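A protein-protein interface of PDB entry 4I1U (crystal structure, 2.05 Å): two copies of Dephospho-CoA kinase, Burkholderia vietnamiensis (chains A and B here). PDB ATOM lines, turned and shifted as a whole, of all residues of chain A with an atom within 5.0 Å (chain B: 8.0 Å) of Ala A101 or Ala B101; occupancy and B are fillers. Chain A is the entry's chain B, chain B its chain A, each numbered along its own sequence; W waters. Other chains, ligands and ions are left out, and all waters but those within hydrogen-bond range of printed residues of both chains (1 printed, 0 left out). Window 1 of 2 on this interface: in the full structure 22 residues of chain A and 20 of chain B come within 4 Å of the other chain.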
ATOM      1  N   PRO A  97     -13.557  16.616 -32.828  1.00  0.00           N
ATOM      2  CA  PRO A  97     -13.827  15.686 -31.735  1.00  0.00           C
ATOM      3  C   PRO A  97     -15.311  15.741 -31.334  1.00  0.00           C
ATOM      4  O   PRO A  97     -15.929  14.716 -31.073  1.00  0.00           O
ATOM      5  CB  PRO A  97     -12.931  16.233 -30.609  1.00  0.00           C
ATOM      6  CG  PRO A  97     -11.773  16.813 -31.351  1.00  0.00           C
ATOM      7  CD  PRO A  97     -12.421  17.495 -32.520  1.00  0.00           C
ATOM      8  N   LEU A  98     -15.872  16.938 -31.297  1.00  0.00           N
ATOM      9  CA  LEU A  98     -17.290  17.079 -30.915  1.00  0.00           C
ATOM     10  C   LEU A  98     -18.221  16.381 -31.903  1.00  0.00           C
ATOM     11  O   LEU A  98     -19.229  15.799 -31.519  1.00  0.00           O
ATOM     12  CB  LEU A  98     -17.659  18.551 -30.764  1.00  0.00           C
ATOM     13  CG  LEU A  98     -17.019  19.197 -29.542  1.00  0.00           C
ATOM     14  CD1 LEU A  98     -17.068  20.706 -29.656  1.00  0.00           C
ATOM     15  CD2 LEU A  98     -17.675  18.715 -28.253  1.00  0.00           C
ATOM     16  N   ILE A  99     -17.892  16.497 -33.185  1.00  0.00           N
ATOM     17  CA  ILE A  99     -18.642  15.807 -34.260  1.00  0.00           C
ATOM     18  C   ILE A  99     -18.584  14.299 -34.053  1.00  0.00           C
ATOM     19  O   ILE A  99     -19.601  13.591 -34.161  1.00  0.00           O
ATOM     20  CB  ILE A  99     -18.118  16.233 -35.660  1.00  0.00           C
ATOM     21  CG1 ILE A  99     -18.506  17.699 -35.925  1.00  0.00           C
ATOM     22  CG2 ILE A  99     -18.707  15.344 -36.740  1.00  0.00           C
ATOM     23  CD1 ILE A  99     -17.745  18.382 -37.042  1.00  0.00           C
ATOM     24  N   ARG A 100     -17.406  13.800 -33.720  1.00  0.00           N
ATOM     25  CA  ARG A 100     -17.272  12.380 -33.448  1.00  0.00           C
ATOM     26  C   ARG A 100     -18.163  11.950 -32.306  1.00  0.00           C
ATOM     27  O   ARG A 100     -18.868  10.958 -32.402  1.00  0.00           O
ATOM     28  CB  ARG A 100     -15.850  12.037 -33.103  1.00  0.00           C
ATOM     29  CG  ARG A 100     -14.854  12.130 -34.223  1.00  0.00           C
ATOM     30  CD  ARG A 100     -13.564  11.496 -33.736  1.00  0.00           C
ATOM     31  NE  ARG A 100     -12.492  11.581 -34.697  1.00  0.00           N
ATOM     32  CZ  ARG A 100     -11.387  10.835 -34.649  1.00  0.00           C
ATOM     33  NH1 ARG A 100     -11.197   9.912 -33.689  1.00  0.00           N
ATOM     34  NH2 ARG A 100     -10.473  10.995 -35.593  1.00  0.00           N
ATOM     35  N   ALA A 101     -18.123  12.696 -31.209  1.00  0.00           N
ATOM     36  CA  ALA A 101     -18.908  12.332 -30.037  1.00  0.00           C
ATOM     37  C   ALA A 101     -20.404  12.398 -30.343  1.00  0.00           C
ATOM     38  O   ALA A 101     -21.141  11.480 -30.002  1.00  0.00           O
ATOM     39  CB  ALA A 101     -18.549  13.246 -28.844  1.00  0.00           C
ATOM     40  N   GLU A 102     -20.845  13.480 -30.970  1.00  0.00           N
ATOM     41  CA  GLU A 102     -22.263  13.635 -31.288  1.00  0.00           C
ATOM     42  C   GLU A 102     -22.659  12.545 -32.263  1.00  0.00           C
ATOM     43  O   GLU A 102     -23.767  12.013 -32.196  1.00  0.00           O
ATOM     44  CB  GLU A 102     -22.550  14.995 -31.923  1.00  0.00           C
ATOM     45  CG  GLU A 102     -22.479  16.177 -30.957  1.00  0.00           C
ATOM     46  CD  GLU A 102     -23.416  15.994 -29.779  1.00  0.00           C
ATOM     47  OE1 GLU A 102     -24.651  15.906 -29.996  1.00  0.00           O
ATOM     48  OE2 GLU A 102     -22.910  15.875 -28.648  1.00  0.00           O
ATOM     49  N   THR A 103     -21.740  12.182 -33.161  1.00  0.00           N
ATOM     50  CA  THR A 103     -22.046  11.114 -34.117  1.00  0.00           C
ATOM     51  C   THR A 103     -22.297   9.842 -33.356  1.00  0.00           C
ATOM     52  O   THR A 103     -23.267   9.142 -33.641  1.00  0.00           O
ATOM     53  CB  THR A 103     -20.920  10.916 -35.176  1.00  0.00           C
ATOM     54  OG1 THR A 103     -20.926  12.035 -36.057  1.00  0.00           O
ATOM     55  CG2 THR A 103     -21.139   9.670 -35.960  1.00  0.00           C
ATOM     56  N   GLU A 104     -21.450   9.531 -32.375  1.00  0.00           N
ATOM     57  CA  GLU A 104     -21.638   8.296 -31.611  1.00  0.00           C
ATOM     58  C   GLU A 104     -22.910   8.345 -30.760  1.00  0.00           C
ATOM     59  O   GLU A 104     -23.601   7.340 -30.624  1.00  0.00           O
ATOM     60  CB  GLU A 104     -20.405   7.942 -30.784  1.00  0.00           C
ATOM     61  CG  GLU A 104     -19.153   7.687 -31.601  1.00  0.00           C
ATOM     62  CD  GLU A 104     -19.154   6.375 -32.390  1.00  0.00           C
ATOM     63  OE1 GLU A 104     -20.128   5.583 -32.350  1.00  0.00           O
ATOM     64  OE2 GLU A 104     -18.111   6.099 -33.026  1.00  0.00           O
ATOM     65  N   ARG A 105     -23.225   9.512 -30.199  1.00  0.00           N
ATOM     66  CA  ARG A 105     -24.455   9.685 -29.413  1.00  0.00           C
ATOM     67  C   ARG A 105     -25.673   9.343 -30.254  1.00  0.00           C
ATOM     68  O   ARG A 105     -26.513   8.569 -29.846  1.00  0.00           O
ATOM     69  CB  ARG A 105     -24.584  11.129 -28.873  1.00  0.00           C
ATOM     70  CG  ARG A 105     -23.757  11.365 -27.630  1.00  0.00           C
ATOM     71  CD  ARG A 105     -23.966  12.744 -26.970  1.00  0.00           C
ATOM     72  NE  ARG A 105     -23.010  12.831 -25.857  1.00  0.00           N
ATOM     73  CZ  ARG A 105     -23.187  12.229 -24.674  1.00  0.00           C
ATOM     74  NH1 ARG A 105     -24.288  11.523 -24.439  1.00  0.00           N
ATOM     75  NH2 ARG A 105     -22.270  12.318 -23.709  1.00  0.00           N
ATOM     76  N   ILE B  42     -13.743  10.499 -17.325  1.00  0.00           N
ATOM     77  CA  ILE B  42     -14.314  10.502 -18.679  1.00  0.00           C
ATOM     78  C   ILE B  42     -13.773   9.353 -19.528  1.00  0.00           C
ATOM     79  O   ILE B  42     -14.548   8.644 -20.173  1.00  0.00           O
ATOM     80  CB  ILE B  42     -14.087  11.863 -19.355  1.00  0.00           C
ATOM     81  CG1 ILE B  42     -14.825  12.946 -18.551  1.00  0.00           C
ATOM     82  CG2 ILE B  42     -14.597  11.786 -20.778  1.00  0.00           C
ATOM     83  CD1 ILE B  42     -14.715  14.367 -19.105  1.00  0.00           C
ATOM     84  N   ILE B  46     -16.272   6.542 -21.131  1.00  0.00           N
ATOM     85  CA  ILE B  46     -16.455   6.272 -22.557  1.00  0.00           C
ATOM     86  C   ILE B  46     -16.029   4.858 -22.977  1.00  0.00           C
ATOM     87  O   ILE B  46     -16.292   4.465 -24.108  1.00  0.00           O
ATOM     88  CB  ILE B  46     -15.755   7.285 -23.457  1.00  0.00           C
ATOM     89  CG1 ILE B  46     -14.251   7.265 -23.273  1.00  0.00           C
ATOM     90  CG2 ILE B  46     -16.362   8.661 -23.265  1.00  0.00           C
ATOM     91  CD1 ILE B  46     -13.559   8.180 -24.270  1.00  0.00           C
ATOM     92  N   LEU B  52     -19.040   5.781 -25.491  1.00  0.00           N
ATOM     93  CA  LEU B  52     -18.925   6.313 -26.849  1.00  0.00           C
ATOM     94  C   LEU B  52     -17.718   5.774 -27.618  1.00  0.00           C
ATOM     95  O   LEU B  52     -17.679   5.854 -28.868  1.00  0.00           O
ATOM     96  CB  LEU B  52     -18.813   7.836 -26.817  1.00  0.00           C
ATOM     97  CG  LEU B  52     -20.035   8.561 -26.280  1.00  0.00           C
ATOM     98  CD1 LEU B  52     -19.714  10.031 -26.272  1.00  0.00           C
ATOM     99  CD2 LEU B  52     -21.251   8.294 -27.132  1.00  0.00           C
ATOM    100  N   THR B  95      -9.663   7.512 -28.251  1.00  0.00           N
ATOM    101  CA  THR B  95     -10.176   7.935 -26.931  1.00  0.00           C
ATOM    102  C   THR B  95      -9.908   9.393 -26.714  1.00  0.00           C
ATOM    103  O   THR B  95     -10.765  10.096 -26.164  1.00  0.00           O
ATOM    104  CB  THR B  95      -9.591   7.112 -25.755  1.00  0.00           C
ATOM    105  OG1 THR B  95      -8.184   7.094 -25.842  1.00  0.00           O
ATOM    106  CG2 THR B  95     -10.065   5.711 -25.784  1.00  0.00           C
ATOM    107  N   HIS B  96      -8.741   9.859 -27.131  1.00  0.00           N
ATOM    108  CA  HIS B  96      -8.361  11.244 -26.863  1.00  0.00           C
ATOM    109  C   HIS B  96      -9.298  12.320 -27.421  1.00  0.00           C
ATOM    110  O   HIS B  96      -9.637  13.269 -26.694  1.00  0.00           O
ATOM    111  CB  HIS B  96      -6.909  11.511 -27.253  1.00  0.00           C
ATOM    112  CG  HIS B  96      -5.924  10.903 -26.302  1.00  0.00           C
ATOM    113  ND1 HIS B  96      -4.594  11.248 -26.284  1.00  0.00           N
ATOM    114  CD2 HIS B  96      -6.090  10.003 -25.303  1.00  0.00           C
ATOM    115  CE1 HIS B  96      -3.976  10.563 -25.335  1.00  0.00           C
ATOM    116  NE2 HIS B  96      -4.866   9.814 -24.714  1.00  0.00           N
ATOM    117  N   PRO B  97      -9.723  12.193 -28.697  1.00  0.00           N
ATOM    118  CA  PRO B  97     -10.713  13.166 -29.176  1.00  0.00           C
ATOM    119  C   PRO B  97     -12.032  13.066 -28.417  1.00  0.00           C
ATOM    120  O   PRO B  97     -12.673  14.075 -28.143  1.00  0.00           O
ATOM    121  CB  PRO B  97     -10.958  12.756 -30.640  1.00  0.00           C
ATOM    122  CG  PRO B  97      -9.753  11.934 -31.031  1.00  0.00           C
ATOM    123  CD  PRO B  97      -9.188  11.335 -29.767  1.00  0.00           C
ATOM    124  N   LEU B  98     -12.456  11.851 -28.116  1.00  0.00           N
ATOM    125  CA  LEU B  98     -13.702  11.687 -27.402  1.00  0.00           C
ATOM    126  C   LEU B  98     -13.605  12.257 -25.971  1.00  0.00           C
ATOM    127  O   LEU B  98     -14.557  12.862 -25.478  1.00  0.00           O
ATOM    128  CB  LEU B  98     -14.137  10.242 -27.385  1.00  0.00           C
ATOM    129  CG  LEU B  98     -14.640   9.694 -28.720  1.00  0.00           C
ATOM    130  CD1 LEU B  98     -14.962   8.244 -28.518  1.00  0.00           C
ATOM    131  CD2 LEU B  98     -15.883  10.394 -29.230  1.00  0.00           C
ATOM    132  N   ILE B  99     -12.466  12.090 -25.333  1.00  0.00           N
ATOM    133  CA  ILE B  99     -12.264  12.645 -23.968  1.00  0.00           C
ATOM    134  C   ILE B  99     -12.360  14.183 -24.042  1.00  0.00           C
ATOM    135  O   ILE B  99     -13.070  14.836 -23.252  1.00  0.00           O
ATOM    136  CB  ILE B  99     -10.919  12.177 -23.386  1.00  0.00           C
ATOM    137  CG1 ILE B  99     -10.989  10.686 -23.033  1.00  0.00           C
ATOM    138  CG2 ILE B  99     -10.558  13.006 -22.159  1.00  0.00           C
ATOM    139  CD1 ILE B  99      -9.629  10.038 -22.884  1.00  0.00           C
ATOM    140  N   ARG B 100     -11.671  14.763 -25.017  1.00  0.00           N
ATOM    141  CA  ARG B 100     -11.678  16.206 -25.184  1.00  0.00           C
ATOM    142  C   ARG B 100     -13.100  16.681 -25.437  1.00  0.00           C
ATOM    143  O   ARG B 100     -13.536  17.677 -24.859  1.00  0.00           O
ATOM    144  CB  ARG B 100     -10.688  16.684 -26.262  1.00  0.00           C
ATOM    145  CG  ARG B 100      -9.203  16.608 -25.842  1.00  0.00           C
ATOM    146  CD  ARG B 100      -8.290  17.472 -26.737  1.00  0.00           C
ATOM    147  NE  ARG B 100      -8.274  16.952 -28.082  1.00  0.00           N
ATOM    148  CZ  ARG B 100      -7.565  15.884 -28.503  1.00  0.00           C
ATOM    149  NH1 ARG B 100      -6.680  15.259 -27.713  1.00  0.00           N
ATOM    150  NH2 ARG B 100      -7.694  15.478 -29.766  1.00  0.00           N
ATOM    151  N   ALA B 101     -13.854  15.946 -26.231  1.00  0.00           N
ATOM    152  CA  ALA B 101     -15.216  16.352 -26.541  1.00  0.00           C
ATOM    153  C   ALA B 101     -16.138  16.293 -25.328  1.00  0.00           C
ATOM    154  O   ALA B 101     -16.893  17.237 -25.056  1.00  0.00           O
ATOM    155  CB  ALA B 101     -15.785  15.496 -27.670  1.00  0.00           C
ATOM    156  N   GLU B 102     -16.118  15.158 -24.646  1.00  0.00           N
ATOM    157  CA  GLU B 102     -16.959  14.945 -23.486  1.00  0.00           C
ATOM    158  C   GLU B 102     -16.625  15.890 -22.333  1.00  0.00           C
ATOM    159  O   GLU B 102     -17.512  16.237 -21.511  1.00  0.00           O
ATOM    160  CB  GLU B 102     -16.851  13.491 -23.025  1.00  0.00           C
ATOM    161  CG  GLU B 102     -17.574  12.527 -23.956  1.00  0.00           C
ATOM    162  CD  GLU B 102     -19.054  12.877 -24.081  1.00  0.00           C
ATOM    163  OE1 GLU B 102     -19.783  12.588 -23.104  1.00  0.00           O
ATOM    164  OE2 GLU B 102     -19.458  13.502 -25.116  1.00  0.00           O
ATOM    165  N   THR B 103     -15.362  16.316 -22.285  1.00  0.00           N
ATOM    166  CA  THR B 103     -14.947  17.358 -21.360  1.00  0.00           C
ATOM    167  C   THR B 103     -15.821  18.611 -21.552  1.00  0.00           C
ATOM    168  O   THR B 103     -16.235  19.229 -20.571  1.00  0.00           O
ATOM    169  CB  THR B 103     -13.430  17.670 -21.491  1.00  0.00           C
ATOM    170  OG1 THR B 103     -12.679  16.571 -20.980  1.00  0.00           O
ATOM    171  CG2 THR B 103     -13.053  18.883 -20.701  1.00  0.00           C
ATOM    172  N   GLU B 104     -16.144  18.976 -22.801  1.00  0.00           N
ATOM    173  CA  GLU B 104     -16.947  20.176 -23.032  1.00  0.00           C
ATOM    174  C   GLU B 104     -18.336  20.007 -22.540  1.00  0.00           C
ATOM    175  O   GLU B 104     -18.946  20.955 -22.043  1.00  0.00           O
ATOM    176  CB  GLU B 104     -17.022  20.597 -24.514  1.00  0.00           C
ATOM    177  CG  GLU B 104     -15.700  20.936 -25.141  1.00  0.00           C
ATOM    178  CD  GLU B 104     -15.009  22.111 -24.483  1.00  0.00           C
ATOM    179  OE1 GLU B 104     -15.662  23.101 -24.049  1.00  0.00           O
ATOM    180  OE2 GLU B 104     -13.765  22.044 -24.438  1.00  0.00           O
ATOM    181  N   ARG B 105     -18.871  18.819 -22.714  1.00  0.00           N
ATOM    182  CA  ARG B 105     -20.205  18.567 -22.290  1.00  0.00           C
ATOM    183  C   ARG B 105     -20.319  18.649 -20.763  1.00  0.00           C
ATOM    184  O   ARG B 105     -21.299  19.202 -20.240  1.00  0.00           O
ATOM    185  CB  ARG B 105     -20.592  17.172 -22.782  1.00  0.00           C
ATOM    186  CG  ARG B 105     -22.053  16.825 -22.799  1.00  0.00           C
ATOM    187  CD  ARG B 105     -22.267  15.485 -23.523  1.00  0.00           C
ATOM    188  NE  ARG B 105     -22.721  15.676 -24.896  1.00  0.00           N
ATOM    189  CZ  ARG B 105     -23.991  15.937 -25.227  1.00  0.00           C
ATOM    190  NH1 ARG B 105     -24.322  16.132 -26.492  1.00  0.00           N
ATOM    191  NH2 ARG B 105     -24.952  16.023 -24.292  1.00  0.00           N
ATOM    192  N   GLU B 106     -19.345  18.042 -20.060  1.00  0.00           N
ATOM    193  CA  GLU B 106     -19.311  18.085 -18.601  1.00  0.00           C
ATOM    194  C   GLU B 106     -19.063  19.510 -18.137  1.00  0.00           C
ATOM    195  O   GLU B 106     -19.720  19.960 -17.209  1.00  0.00           O
ATOM    196  CB  GLU B 106     -18.256  17.119 -18.005  1.00  0.00           C
ATOM    197  CG  GLU B 106     -18.478  15.639 -18.328  1.00  0.00           C
ATOM    198  CD  GLU B 106     -18.807  14.672 -17.151  1.00  0.00           C
ATOM    199  OE1 GLU B 106     -19.181  15.079 -16.027  1.00  0.00           O
ATOM    200  OE2 GLU B 106     -18.689  13.425 -17.378  1.00  0.00           O
ATOM    201  N   ALA B 107     -18.168  20.252 -18.794  1.00  0.00           N
ATOM    202  CA  ALA B 107     -17.877  21.612 -18.356  1.00  0.00           C
ATOM    203  C   ALA B 107     -19.091  22.546 -18.464  1.00  0.00           C
ATOM    204  O   ALA B 107     -19.221  23.452 -17.664  1.00  0.00           O
ATOM    205  CB  ALA B 107     -16.719  22.227 -19.125  1.00  0.00           C
ATOM    206  N   TRP B 128      -4.975  21.299 -25.365  1.00  0.00           N
ATOM    207  CA  TRP B 128      -5.245  21.594 -23.964  1.00  0.00           C
ATOM    208  C   TRP B 128      -4.707  22.940 -23.502  1.00  0.00           C
ATOM    209  O   TRP B 128      -5.403  23.664 -22.802  1.00  0.00           O
ATOM    210  CB  TRP B 128      -4.729  20.494 -23.068  1.00  0.00           C
ATOM    211  CG  TRP B 128      -5.589  19.300 -23.073  1.00  0.00           C
ATOM    212  CD1 TRP B 128      -5.275  18.077 -23.584  1.00  0.00           C
ATOM    213  CD2 TRP B 128      -6.890  19.183 -22.519  1.00  0.00           C
ATOM    214  NE1 TRP B 128      -6.314  17.214 -23.398  1.00  0.00           N
ATOM    215  CE2 TRP B 128      -7.322  17.868 -22.748  1.00  0.00           C
ATOM    216  CE3 TRP B 128      -7.757  20.073 -21.870  1.00  0.00           C
ATOM    217  CZ2 TRP B 128      -8.581  17.406 -22.331  1.00  0.00           C
ATOM    218  CZ3 TRP B 128      -8.991  19.623 -21.468  1.00  0.00           C
ATOM    219  CH2 TRP B 128      -9.400  18.301 -21.717  1.00  0.00           C
HETATM  220  O   HOH W   1     -16.542   4.872 -31.165  1.00  0.00           O
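Among the printed residues, pairs that only touch across the chains: Pro A97 with Pro B97 (3.3 Å), Pro A97 with Ala B101 (3.5 Å), Glu A104 with Leu B52 (3.6 Å), Leu A98 with Ala B101 (3.6 Å), Arg A100 with Pro B97 (3.6 Å), Ala A101 with Leu B98 (3.7 Å), Ala A101 with Ala B101 (3.8 Å), Arg A105 with Leu B52 (3.8 Å) and Ala A101 with Glu B102 (3.8 Å).
The guanidinium group of Arg A105 sits close to the guanidinium group of Arg B105 (3.0 Å).
The guanidinium group (NH2) of Arg A105 lies within salt-bridge range of the side-chain carboxylate (OE1) of Glu B102.
NH1 of Arg B105 is in salt-bridge range of OE2 of Glu A102.
The backbone carbonyl oxygen of Ile B46 is in hydrogen-bond range of the backbone NH of Leu B52.
The guanidinium group (NE) of Arg B105 is in salt-bridge range of the side-chain carboxylate (OE2) of Glu B102 (3.9 Å).
Printed residues of chain B within 4 Å of Leu A98: Ala B101 (3.6 Å).
Ala A101 touches just these residues of chain B: Leu B98 (3.7 Å), Ala B101 (3.8 Å) and Glu B102 (3.8 Å).
Thr A103 touches none of the printed residues of chain B.
Of the printed residues of chain B, Arg A105 touches Leu B52, Glu B102 and Arg B105.
Of the printed residues of chain A, Leu B52 touches Glu A104 and Arg A105.
Printed residues of chain A within 4 Å of Ala B101: Pro A97, Leu A98 and Ala A101.
Of the printed residues of chain A, Arg B105 touches Glu A102 and Arg A105.
The nearest residue of chain B that does not touch Ala A101 is Leu B52 (4.2 Å).
The nearest printed residue of chain B that does not touch Leu A98 is Glu B104 (4.2 Å).
Hydrophobic or aromatic side chains of chain A that line the printed part of chain B: Pro A97, Leu A98 and Ala A101.
Of the 17 printed residues of chain B, 6 touch a printed residue of chain A.
Among the printed residues, 12 pairs touch across the chains.
Among the printed residues, Asp or Glu carboxylates within 4 Å of a Lys or Arg side-chain nitrogen of the other chain: Glu A102 with Arg B105 (2.6 Å) and Arg A105 with Glu B102 (2.6 Å).
Water W1 lies within hydrogen-bond range of OE2 of Glu A104 (2.7 Å) and O of Leu B52 (2.7 Å).
Pro A97 touches its own counterpart, Pro B97.
Leu A98 touches Ala B101, and with the chains exchanged Ala A101 touches Leu B98.
Ala A101 touches Glu B102, but with the chains exchanged Glu A102 does not touch Ala B101 (6.4 Å).
Arg A105 touches its own counterpart, Arg B105.
Positions printed for both chains: 97, 98, 99, 100, 101, 102, 103, 104 and 105.
Of the 12 pairs that touch across the chains among the printed residues, 7 have their exchanged pair printed and touching as well.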
